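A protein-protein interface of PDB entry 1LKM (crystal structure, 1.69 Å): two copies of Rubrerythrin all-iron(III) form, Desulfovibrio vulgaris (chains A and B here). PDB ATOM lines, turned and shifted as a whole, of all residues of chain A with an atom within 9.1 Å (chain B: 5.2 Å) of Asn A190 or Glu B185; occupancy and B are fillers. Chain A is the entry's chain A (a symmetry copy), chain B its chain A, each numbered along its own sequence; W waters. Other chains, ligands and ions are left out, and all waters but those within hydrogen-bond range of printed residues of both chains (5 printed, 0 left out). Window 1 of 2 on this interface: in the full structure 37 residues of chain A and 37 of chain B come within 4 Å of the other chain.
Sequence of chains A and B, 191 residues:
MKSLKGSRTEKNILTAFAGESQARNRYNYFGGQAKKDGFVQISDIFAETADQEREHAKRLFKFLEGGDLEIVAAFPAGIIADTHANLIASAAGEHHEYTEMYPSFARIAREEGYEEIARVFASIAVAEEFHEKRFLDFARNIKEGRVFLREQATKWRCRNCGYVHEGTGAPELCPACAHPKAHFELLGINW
Among the printed residues, merely in contact across the chains: Gln A52 with Cys B158 (3.7 Å), Phe A130 with Leu B187 (3.4 Å), Arg A134 with Arg B157 (3.6 Å), Asn A190 with Glu B185 (3.6 Å), Asn A190 with Gly B188 (3.7 Å) and Trp A191 with Leu B186 (3.9 Å).
Positions printed for both chains: 157, 185, 187 and 188. Of the 11 pairs that touch across the chains among the printed residues, none has its exchanged pair printed and touching as well.
Hydrophobic or aromatic side chains of chain B that line the printed part of chain A: Leu B186 and Leu B187.
Of chain B, only Gln B41 (3.3 Å), Glu B185 (3.6 Å), Leu B186 (3.2 Å) and Gly B188 (3.7 Å) come within 4 Å of Asn A190. Of chain A, only Asn A190 comes within 4 Å of Glu B185. Of chain A, only Glu A48, Gln A52 and Arg A134 come within 4 Å of Arg B157. Leu B186 touches two residues of chain A. Of the printed residues of chain B, Phe A130 touches Leu B187 (3.4 Å). Printed residues of chain A within 4 Å of Gly B188: Asn A190 (3.7 Å). Printed residues of chain A within 4 Å of Cys B158: Gln A52 (3.7 Å). Lys B155 touches none of the printed residues of chain A. Arg A157 touches none of the printed residues of chain B. The nearest residue of chain B that does not touch Asn A190 is Leu B187 (4.4 Å).
The guanidinium group (NH2) of Arg B157 lies within salt-bridge range of the side-chain carboxylate (OE2) of Glu B185 (3.0 Å). The backbone carbonyl oxygen (O) of His B183 is in hydrogen-bond range of the backbone NH (N) of Arg B159, at 2.9 Å. O of Lys B155 sits at hydrogen-bond distance from N of Leu B187, at 2.9 Å. The side-chain carboxylate (OE1) of Glu A48 is in salt-bridge range of the guanidinium group (NH1) of Arg A134. NH1 of Arg B159 lies within salt-bridge range of OE1 of Glu B185, 2.8 Å away.
OD1 of Asn A190 lies close to O of Leu B186, at 3.2 Å. The side-chain carboxylate (OE1) of Glu A48 is in salt-bridge range of the guanidinium group (NH1) of Arg B157, 2.9 Å away. OE1 of Gln B41 lies close to O of Asn A190, at 3.3 Å. The backbone carbonyl oxygen (O) of Arg B159 lies within hydrogen-bond range of the side-chain amide nitrogen (NE2) of Gln A52. NE2 of Gln A52 lies close to NH1 of Arg B157 (3.3 Å).
Water W5 lies within hydrogen-bond range of the backbone carbonyl oxygen of Arg B159 and the side-chain carboxylate of Glu A48. Water W2 lies within hydrogen-bond range of the side-chain carboxylate (OE2) of Glu A48 (2.8 Å) and the guanidinium group (NH2) of Arg B159 (3.4 Å). Water W1 lies within hydrogen-bond range of NE2 of Gln B41 (2.8 Å), O of Asn A190 (2.9 Å) and N of Leu B186 (3.0 Å). Water W4 lies within hydrogen-bond range of NH1 of Arg B157 (2.8 Å) and OE1 of Gln A52 (2.8 Å). Water W3 lies within hydrogen-bond range of the side-chain carboxylate of Glu B185 (2.9 Å), the side-chain amide oxygen of Asn A190 (3.3 Å) and the guanidinium group of Arg B159 (3.4 Å).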
ATOM      1  N   GLU A  48     -19.604   0.344  10.021  1.00  0.00           N
ATOM      2  CA  GLU A  48     -20.354   1.062  11.046  1.00  0.00           C
ATOM      3  C   GLU A  48     -20.486   2.529  10.666  1.00  0.00           C
ATOM      4  O   GLU A  48     -21.539   3.128  10.847  1.00  0.00           O
ATOM      5  CB  GLU A  48     -19.668   0.968  12.415  1.00  0.00           C
ATOM      6  CG  GLU A  48     -20.492   1.626  13.533  1.00  0.00           C
ATOM      7  CD  GLU A  48     -19.692   1.893  14.798  1.00  0.00           C
ATOM      8  OE1 GLU A  48     -18.776   2.735  14.753  1.00  0.00           O
ATOM      9  OE2 GLU A  48     -19.986   1.268  15.839  1.00  0.00           O
ATOM     10  N   GLN A  52     -23.827   4.812  10.131  1.00  0.00           N
ATOM     11  CA  GLN A  52     -24.080   6.059  10.835  1.00  0.00           C
ATOM     12  C   GLN A  52     -24.362   7.172   9.829  1.00  0.00           C
ATOM     13  O   GLN A  52     -25.171   8.056  10.105  1.00  0.00           O
ATOM     14  CB  GLN A  52     -22.907   6.383  11.775  1.00  0.00           C
ATOM     15  CG  GLN A  52     -22.685   5.240  12.778  1.00  0.00           C
ATOM     16  CD  GLN A  52     -21.671   5.540  13.863  1.00  0.00           C
ATOM     17  OE1 GLN A  52     -20.668   6.211  13.629  1.00  0.00           O
ATOM     18  NE2 GLN A  52     -21.919   5.014  15.062  1.00  0.00           N
ATOM     19  N   PHE A 130     -15.280  12.822  14.989  1.00  0.00           N
ATOM     20  CA  PHE A 130     -14.772  11.579  15.549  1.00  0.00           C
ATOM     21  C   PHE A 130     -14.569  10.567  14.422  1.00  0.00           C
ATOM     22  O   PHE A 130     -13.657   9.742  14.482  1.00  0.00           O
ATOM     23  CB  PHE A 130     -15.706  11.003  16.620  1.00  0.00           C
ATOM     24  CG  PHE A 130     -15.135   9.799  17.325  1.00  0.00           C
ATOM     25  CD1 PHE A 130     -13.957   9.902  18.062  1.00  0.00           C
ATOM     26  CD2 PHE A 130     -15.746   8.555  17.212  1.00  0.00           C
ATOM     27  CE1 PHE A 130     -13.391   8.777  18.675  1.00  0.00           C
ATOM     28  CE2 PHE A 130     -15.190   7.424  17.820  1.00  0.00           C
ATOM     29  CZ  PHE A 130     -14.011   7.538  18.551  1.00  0.00           C
ATOM     30  N   ARG A 134     -11.027   8.479  13.857  1.00  0.00           N
ATOM     31  CA  ARG A 134     -10.850   7.041  13.689  1.00  0.00           C
ATOM     32  C   ARG A 134     -10.114   6.728  12.397  1.00  0.00           C
ATOM     33  O   ARG A 134      -9.155   5.960  12.397  1.00  0.00           O
ATOM     34  CB  ARG A 134     -12.196   6.306  13.685  1.00  0.00           C
ATOM     35  CG  ARG A 134     -12.955   6.394  14.990  1.00  0.00           C
ATOM     36  CD  ARG A 134     -13.969   5.259  15.127  1.00  0.00           C
ATOM     37  NE  ARG A 134     -15.002   5.276  14.093  1.00  0.00           N
ATOM     38  CZ  ARG A 134     -16.109   4.540  14.146  1.00  0.00           C
ATOM     39  NH1 ARG A 134     -16.317   3.735  15.180  1.00  0.00           N
ATOM     40  NH2 ARG A 134     -17.015   4.613  13.177  1.00  0.00           N
ATOM     41  N   ARG A 157      -7.626  -9.178  20.957  1.00  0.00           N
ATOM     42  CA  ARG A 157      -8.835  -9.988  20.940  1.00  0.00           C
ATOM     43  C   ARG A 157      -9.193 -10.407  19.524  1.00  0.00           C
ATOM     44  O   ARG A 157      -9.095  -9.613  18.594  1.00  0.00           O
ATOM     45  CB  ARG A 157     -10.017  -9.214  21.538  1.00  0.00           C
ATOM     46  CG  ARG A 157     -11.276 -10.071  21.723  1.00  0.00           C
ATOM     47  CD  ARG A 157     -12.478  -9.250  22.178  1.00  0.00           C
ATOM     48  NE  ARG A 157     -12.989  -8.394  21.109  1.00  0.00           N
ATOM     49  CZ  ARG A 157     -14.228  -8.453  20.630  1.00  0.00           C
ATOM     50  NH1 ARG A 157     -15.095  -9.331  21.126  1.00  0.00           N
ATOM     51  NH2 ARG A 157     -14.601  -7.640  19.650  1.00  0.00           N
ATOM     52  N   GLU A 185      -7.694  -7.414  17.127  1.00  0.00           N
ATOM     53  CA  GLU A 185      -7.728  -5.999  17.471  1.00  0.00           C
ATOM     54  C   GLU A 185      -7.230  -5.867  18.902  1.00  0.00           C
ATOM     55  O   GLU A 185      -7.136  -6.856  19.630  1.00  0.00           O
ATOM     56  CB  GLU A 185      -9.165  -5.469  17.418  1.00  0.00           C
ATOM     57  CG  GLU A 185     -10.102  -6.213  18.371  1.00  0.00           C
ATOM     58  CD  GLU A 185     -11.515  -5.657  18.388  1.00  0.00           C
ATOM     59  OE1 GLU A 185     -11.913  -5.011  17.399  1.00  0.00           O
ATOM     60  OE2 GLU A 185     -12.235  -5.887  19.387  1.00  0.00           O
ATOM     61  N   LEU A 187      -7.589  -5.399  22.617  1.00  0.00           N
ATOM     62  CA  LEU A 187      -8.727  -5.657  23.489  1.00  0.00           C
ATOM     63  C   LEU A 187      -9.231  -4.324  24.024  1.00  0.00           C
ATOM     64  O   LEU A 187      -8.467  -3.548  24.596  1.00  0.00           O
ATOM     65  CB  LEU A 187      -8.312  -6.559  24.655  1.00  0.00           C
ATOM     66  CG  LEU A 187      -9.365  -7.002  25.683  1.00  0.00           C
ATOM     67  CD1 LEU A 187      -9.839  -5.825  26.516  1.00  0.00           C
ATOM     68  CD2 LEU A 187     -10.528  -7.662  24.970  1.00  0.00           C
ATOM     69  N   GLY A 188     -10.518  -4.065  23.834  1.00  0.00           N
ATOM     70  CA  GLY A 188     -11.090  -2.822  24.305  1.00  0.00           C
ATOM     71  C   GLY A 188     -12.153  -3.027  25.363  1.00  0.00           C
ATOM     72  O   GLY A 188     -12.888  -4.011  25.343  1.00  0.00           O
ATOM     73  N   ILE A 189     -12.224  -2.092  26.301  1.00  0.00           N
ATOM     74  CA  ILE A 189     -13.210  -2.149  27.365  1.00  0.00           C
ATOM     75  C   ILE A 189     -13.808  -0.757  27.534  1.00  0.00           C
ATOM     76  O   ILE A 189     -13.190   0.119  28.133  1.00  0.00           O
ATOM     77  CB  ILE A 189     -12.572  -2.598  28.702  1.00  0.00           C
ATOM     78  CG1 ILE A 189     -12.111  -4.053  28.589  1.00  0.00           C
ATOM     79  CG2 ILE A 189     -13.574  -2.442  29.841  1.00  0.00           C
ATOM     80  CD1 ILE A 189     -11.477  -4.605  29.852  1.00  0.00           C
ATOM     81  N   ASN A 190     -14.997  -0.547  26.978  1.00  0.00           N
ATOM     82  CA  ASN A 190     -15.652   0.745  27.104  1.00  0.00           C
ATOM     83  C   ASN A 190     -16.962   0.622  27.875  1.00  0.00           C
ATOM     84  O   ASN A 190     -18.049   0.821  27.333  1.00  0.00           O
ATOM     85  CB  ASN A 190     -15.883   1.404  25.729  1.00  0.00           C
ATOM     86  CG  ASN A 190     -16.797   0.596  24.810  1.00  0.00           C
ATOM     87  OD1 ASN A 190     -17.501   1.167  23.972  1.00  0.00           O
ATOM     88  ND2 ASN A 190     -16.772  -0.722  24.942  1.00  0.00           N
ATOM     89  N   TRP A 191     -16.831   0.283  29.153  1.00  0.00           N
ATOM     90  CA  TRP A 191     -17.969   0.135  30.053  1.00  0.00           C
ATOM     91  C   TRP A 191     -17.476   0.112  31.499  1.00  0.00           C
ATOM     92  O   TRP A 191     -16.250   0.266  31.701  1.00  0.00           O
ATOM     93  CB  TRP A 191     -18.733  -1.154  29.734  1.00  0.00           C
ATOM     94  CG  TRP A 191     -17.901  -2.402  29.839  1.00  0.00           C
ATOM     95  CD1 TRP A 191     -17.524  -3.050  30.981  1.00  0.00           C
ATOM     96  CD2 TRP A 191     -17.327  -3.137  28.753  1.00  0.00           C
ATOM     97  NE1 TRP A 191     -16.752  -4.145  30.674  1.00  0.00           N
ATOM     98  CE2 TRP A 191     -16.614  -4.221  29.312  1.00  0.00           C
ATOM     99  CE3 TRP A 191     -17.347  -2.985  27.360  1.00  0.00           C
ATOM    100  CZ2 TRP A 191     -15.925  -5.149  28.527  1.00  0.00           C
ATOM    101  CZ3 TRP A 191     -16.661  -3.907  26.579  1.00  0.00           C
ATOM    102  CH2 TRP A 191     -15.961  -4.975  27.165  1.00  0.00           C
ATOM    103  OXT TRP A 191     -18.312  -0.058  32.412  1.00  0.00           O
ATOM    104  N   GLN B  41     -26.015  -1.002  23.590  1.00  0.00           N
ATOM    105  CA  GLN B  41     -24.663  -1.552  23.612  1.00  0.00           C
ATOM    106  C   GLN B  41     -24.701  -2.990  24.106  1.00  0.00           C
ATOM    107  O   GLN B  41     -24.083  -3.878  23.517  1.00  0.00           O
ATOM    108  CB  GLN B  41     -23.727  -0.745  24.520  1.00  0.00           C
ATOM    109  CG  GLN B  41     -22.286  -1.249  24.430  1.00  0.00           C
ATOM    110  CD  GLN B  41     -21.339  -0.621  25.435  1.00  0.00           C
ATOM    111  OE1 GLN B  41     -20.118  -0.711  25.287  1.00  0.00           O
ATOM    112  NE2 GLN B  41     -21.891   0.002  26.468  1.00  0.00           N
ATOM    113  N   LYS B 155     -16.882  10.972  28.142  1.00  0.00           N
ATOM    114  CA  LYS B 155     -17.422  11.062  26.790  1.00  0.00           C
ATOM    115  C   LYS B 155     -18.332   9.888  26.477  1.00  0.00           C
ATOM    116  O   LYS B 155     -17.996   8.737  26.753  1.00  0.00           O
ATOM    117  CB  LYS B 155     -16.290  11.135  25.762  1.00  0.00           C
ATOM    118  CG  LYS B 155     -15.480  12.426  25.841  1.00  0.00           C
ATOM    119  CD  LYS B 155     -14.441  12.503  24.736  1.00  0.00           C
ATOM    120  CE  LYS B 155     -13.666  13.811  24.804  1.00  0.00           C
ATOM    121  NZ  LYS B 155     -12.665  13.915  23.706  1.00  0.00           N
ATOM    122  N   TRP B 156     -19.492  10.200  25.909  1.00  0.00           N
ATOM    123  CA  TRP B 156     -20.476   9.193  25.533  1.00  0.00           C
ATOM    124  C   TRP B 156     -20.669   9.239  24.025  1.00  0.00           C
ATOM    125  O   TRP B 156     -20.716  10.318  23.436  1.00  0.00           O
ATOM    126  CB  TRP B 156     -21.814   9.474  26.216  1.00  0.00           C
ATOM    127  CG  TRP B 156     -21.729   9.522  27.703  1.00  0.00           C
ATOM    128  CD1 TRP B 156     -21.341  10.583  28.476  1.00  0.00           C
ATOM    129  CD2 TRP B 156     -22.012   8.450  28.605  1.00  0.00           C
ATOM    130  NE1 TRP B 156     -21.369  10.235  29.806  1.00  0.00           N
ATOM    131  CE2 TRP B 156     -21.777   8.931  29.914  1.00  0.00           C
ATOM    132  CE3 TRP B 156     -22.443   7.128  28.435  1.00  0.00           C
ATOM    133  CZ2 TRP B 156     -21.958   8.131  31.048  1.00  0.00           C
ATOM    134  CZ3 TRP B 156     -22.622   6.332  29.564  1.00  0.00           C
ATOM    135  CH2 TRP B 156     -22.379   6.839  30.854  1.00  0.00           C
ATOM    136  N   ARG B 157     -20.786   8.074  23.400  1.00  0.00           N
ATOM    137  CA  ARG B 157     -20.971   8.027  21.958  1.00  0.00           C
ATOM    138  C   ARG B 157     -22.308   7.404  21.597  1.00  0.00           C
ATOM    139  O   ARG B 157     -22.720   6.417  22.198  1.00  0.00           O
ATOM    140  CB  ARG B 157     -19.853   7.213  21.292  1.00  0.00           C
ATOM    141  CG  ARG B 157     -19.880   7.280  19.760  1.00  0.00           C
ATOM    142  CD  ARG B 157     -18.857   6.349  19.117  1.00  0.00           C
ATOM    143  NE  ARG B 157     -19.238   4.945  19.251  1.00  0.00           N
ATOM    144  CZ  ARG B 157     -19.436   4.121  18.226  1.00  0.00           C
ATOM    145  NH1 ARG B 157     -19.287   4.559  16.979  1.00  0.00           N
ATOM    146  NH2 ARG B 157     -19.790   2.861  18.444  1.00  0.00           N
ATOM    147  N   CYS B 158     -22.989   7.996  20.621  1.00  0.00           N
ATOM    148  CA  CYS B 158     -24.261   7.462  20.157  1.00  0.00           C
ATOM    149  C   CYS B 158     -23.913   6.347  19.175  1.00  0.00           C
ATOM    150  O   CYS B 158     -23.230   6.587  18.179  1.00  0.00           O
ATOM    151  CB  CYS B 158     -25.068   8.545  19.435  1.00  0.00           C
ATOM    152  SG  CYS B 158     -26.590   7.916  18.692  1.00  0.00           S
ATOM    153  N   ARG B 159     -24.363   5.126  19.451  1.00  0.00           N
ATOM    154  CA  ARG B 159     -24.062   4.015  18.554  1.00  0.00           C
ATOM    155  C   ARG B 159     -24.802   4.132  17.226  1.00  0.00           C
ATOM    156  O   ARG B 159     -24.365   3.579  16.213  1.00  0.00           O
ATOM    157  CB  ARG B 159     -24.404   2.678  19.224  1.00  0.00           C
ATOM    158  CG  ARG B 159     -23.452   2.288  20.354  1.00  0.00           C
ATOM    159  CD  ARG B 159     -23.821   0.938  20.952  1.00  0.00           C
ATOM    160  NE  ARG B 159     -23.740  -0.143  19.973  1.00  0.00           N
ATOM    161  CZ  ARG B 159     -22.604  -0.656  19.507  1.00  0.00           C
ATOM    162  NH1 ARG B 159     -21.432  -0.195  19.929  1.00  0.00           N
ATOM    163  NH2 ARG B 159     -22.641  -1.626  18.605  1.00  0.00           N
ATOM    164  N   HIS B 183     -29.211   4.288  23.047  1.00  0.00           N
ATOM    165  CA  HIS B 183     -28.159   4.075  22.056  1.00  0.00           C
ATOM    166  C   HIS B 183     -26.752   4.494  22.472  1.00  0.00           C
ATOM    167  O   HIS B 183     -25.786   4.186  21.774  1.00  0.00           O
ATOM    168  CB  HIS B 183     -28.542   4.783  20.753  1.00  0.00           C
ATOM    169  CG  HIS B 183     -29.719   4.169  20.064  1.00  0.00           C
ATOM    170  ND1 HIS B 183     -29.588   3.228  19.064  1.00  0.00           N
ATOM    171  CD2 HIS B 183     -31.048   4.309  20.277  1.00  0.00           C
ATOM    172  CE1 HIS B 183     -30.787   2.815  18.694  1.00  0.00           C
ATOM    173  NE2 HIS B 183     -31.690   3.455  19.415  1.00  0.00           N
ATOM    174  N   PHE B 184     -26.623   5.170  23.609  1.00  0.00           N
ATOM    175  CA  PHE B 184     -25.314   5.634  24.057  1.00  0.00           C
ATOM    176  C   PHE B 184     -24.450   4.645  24.835  1.00  0.00           C
ATOM    177  O   PHE B 184     -24.946   3.764  25.533  1.00  0.00           O
ATOM    178  CB  PHE B 184     -25.459   6.918  24.881  1.00  0.00           C
ATOM    179  CG  PHE B 184     -25.774   8.133  24.056  1.00  0.00           C
ATOM    180  CD1 PHE B 184     -27.088   8.440  23.714  1.00  0.00           C
ATOM    181  CD2 PHE B 184     -24.750   8.961  23.601  1.00  0.00           C
ATOM    182  CE1 PHE B 184     -27.378   9.560  22.928  1.00  0.00           C
ATOM    183  CE2 PHE B 184     -25.025  10.081  22.815  1.00  0.00           C
ATOM    184  CZ  PHE B 184     -26.344  10.381  22.478  1.00  0.00           C
ATOM    185  N   GLU B 185     -23.139   4.822  24.694  1.00  0.00           N
ATOM    186  CA  GLU B 185     -22.138   4.001  25.362  1.00  0.00           C
ATOM    187  C   GLU B 185     -20.957   4.900  25.690  1.00  0.00           C
ATOM    188  O   GLU B 185     -20.850   6.013  25.173  1.00  0.00           O
ATOM    189  CB  GLU B 185     -21.644   2.891  24.428  1.00  0.00           C
ATOM    190  CG  GLU B 185     -21.027   3.439  23.140  1.00  0.00           C
ATOM    191  CD  GLU B 185     -20.466   2.360  22.231  1.00  0.00           C
ATOM    192  OE1 GLU B 185     -20.906   1.199  22.342  1.00  0.00           O
ATOM    193  OE2 GLU B 185     -19.596   2.681  21.389  1.00  0.00           O
ATOM    194  N   LEU B 186     -20.069   4.427  26.555  1.00  0.00           N
ATOM    195  CA  LEU B 186     -18.882   5.205  26.867  1.00  0.00           C
ATOM    196  C   LEU B 186     -18.053   5.181  25.595  1.00  0.00           C
ATOM    197  O   LEU B 186     -17.919   4.130  24.961  1.00  0.00           O
ATOM    198  CB  LEU B 186     -18.079   4.559  27.999  1.00  0.00           C
ATOM    199  CG  LEU B 186     -18.659   4.643  29.411  1.00  0.00           C
ATOM    200  CD1 LEU B 186     -17.688   3.993  30.388  1.00  0.00           C
ATOM    201  CD2 LEU B 186     -18.888   6.098  29.789  1.00  0.00           C
ATOM    202  N   LEU B 187     -17.511   6.330  25.209  1.00  0.00           N
ATOM    203  CA  LEU B 187     -16.682   6.397  24.013  1.00  0.00           C
ATOM    204  C   LEU B 187     -15.471   5.499  24.219  1.00  0.00           C
ATOM    205  O   LEU B 187     -14.748   5.637  25.205  1.00  0.00           O
ATOM    206  CB  LEU B 187     -16.223   7.836  23.762  1.00  0.00           C
ATOM    207  CG  LEU B 187     -15.370   8.156  22.524  1.00  0.00           C
ATOM    208  CD1 LEU B 187     -13.990   7.537  22.641  1.00  0.00           C
ATOM    209  CD2 LEU B 187     -16.079   7.667  21.277  1.00  0.00           C
ATOM    210  N   GLY B 188     -15.256   4.581  23.286  1.00  0.00           N
ATOM    211  CA  GLY B 188     -14.130   3.679  23.394  1.00  0.00           C
ATOM    212  C   GLY B 188     -13.133   3.843  22.268  1.00  0.00           C
ATOM    213  O   GLY B 188     -13.497   4.151  21.136  1.00  0.00           O
HETATM  214  O   HOH W   1     -20.590   1.905  28.053  1.00  0.00           O
HETATM  215  O   HOH W   2     -20.816  -1.384  15.777  1.00  0.00           O
HETATM  216  O   HOH W   3     -18.225   0.156  20.946  1.00  0.00           O
HETATM  217  O   HOH W   4     -18.570   6.810  15.456  1.00  0.00           O
HETATM  218  O   HOH W   5     -23.170   1.090  16.091  1.00  0.00           O
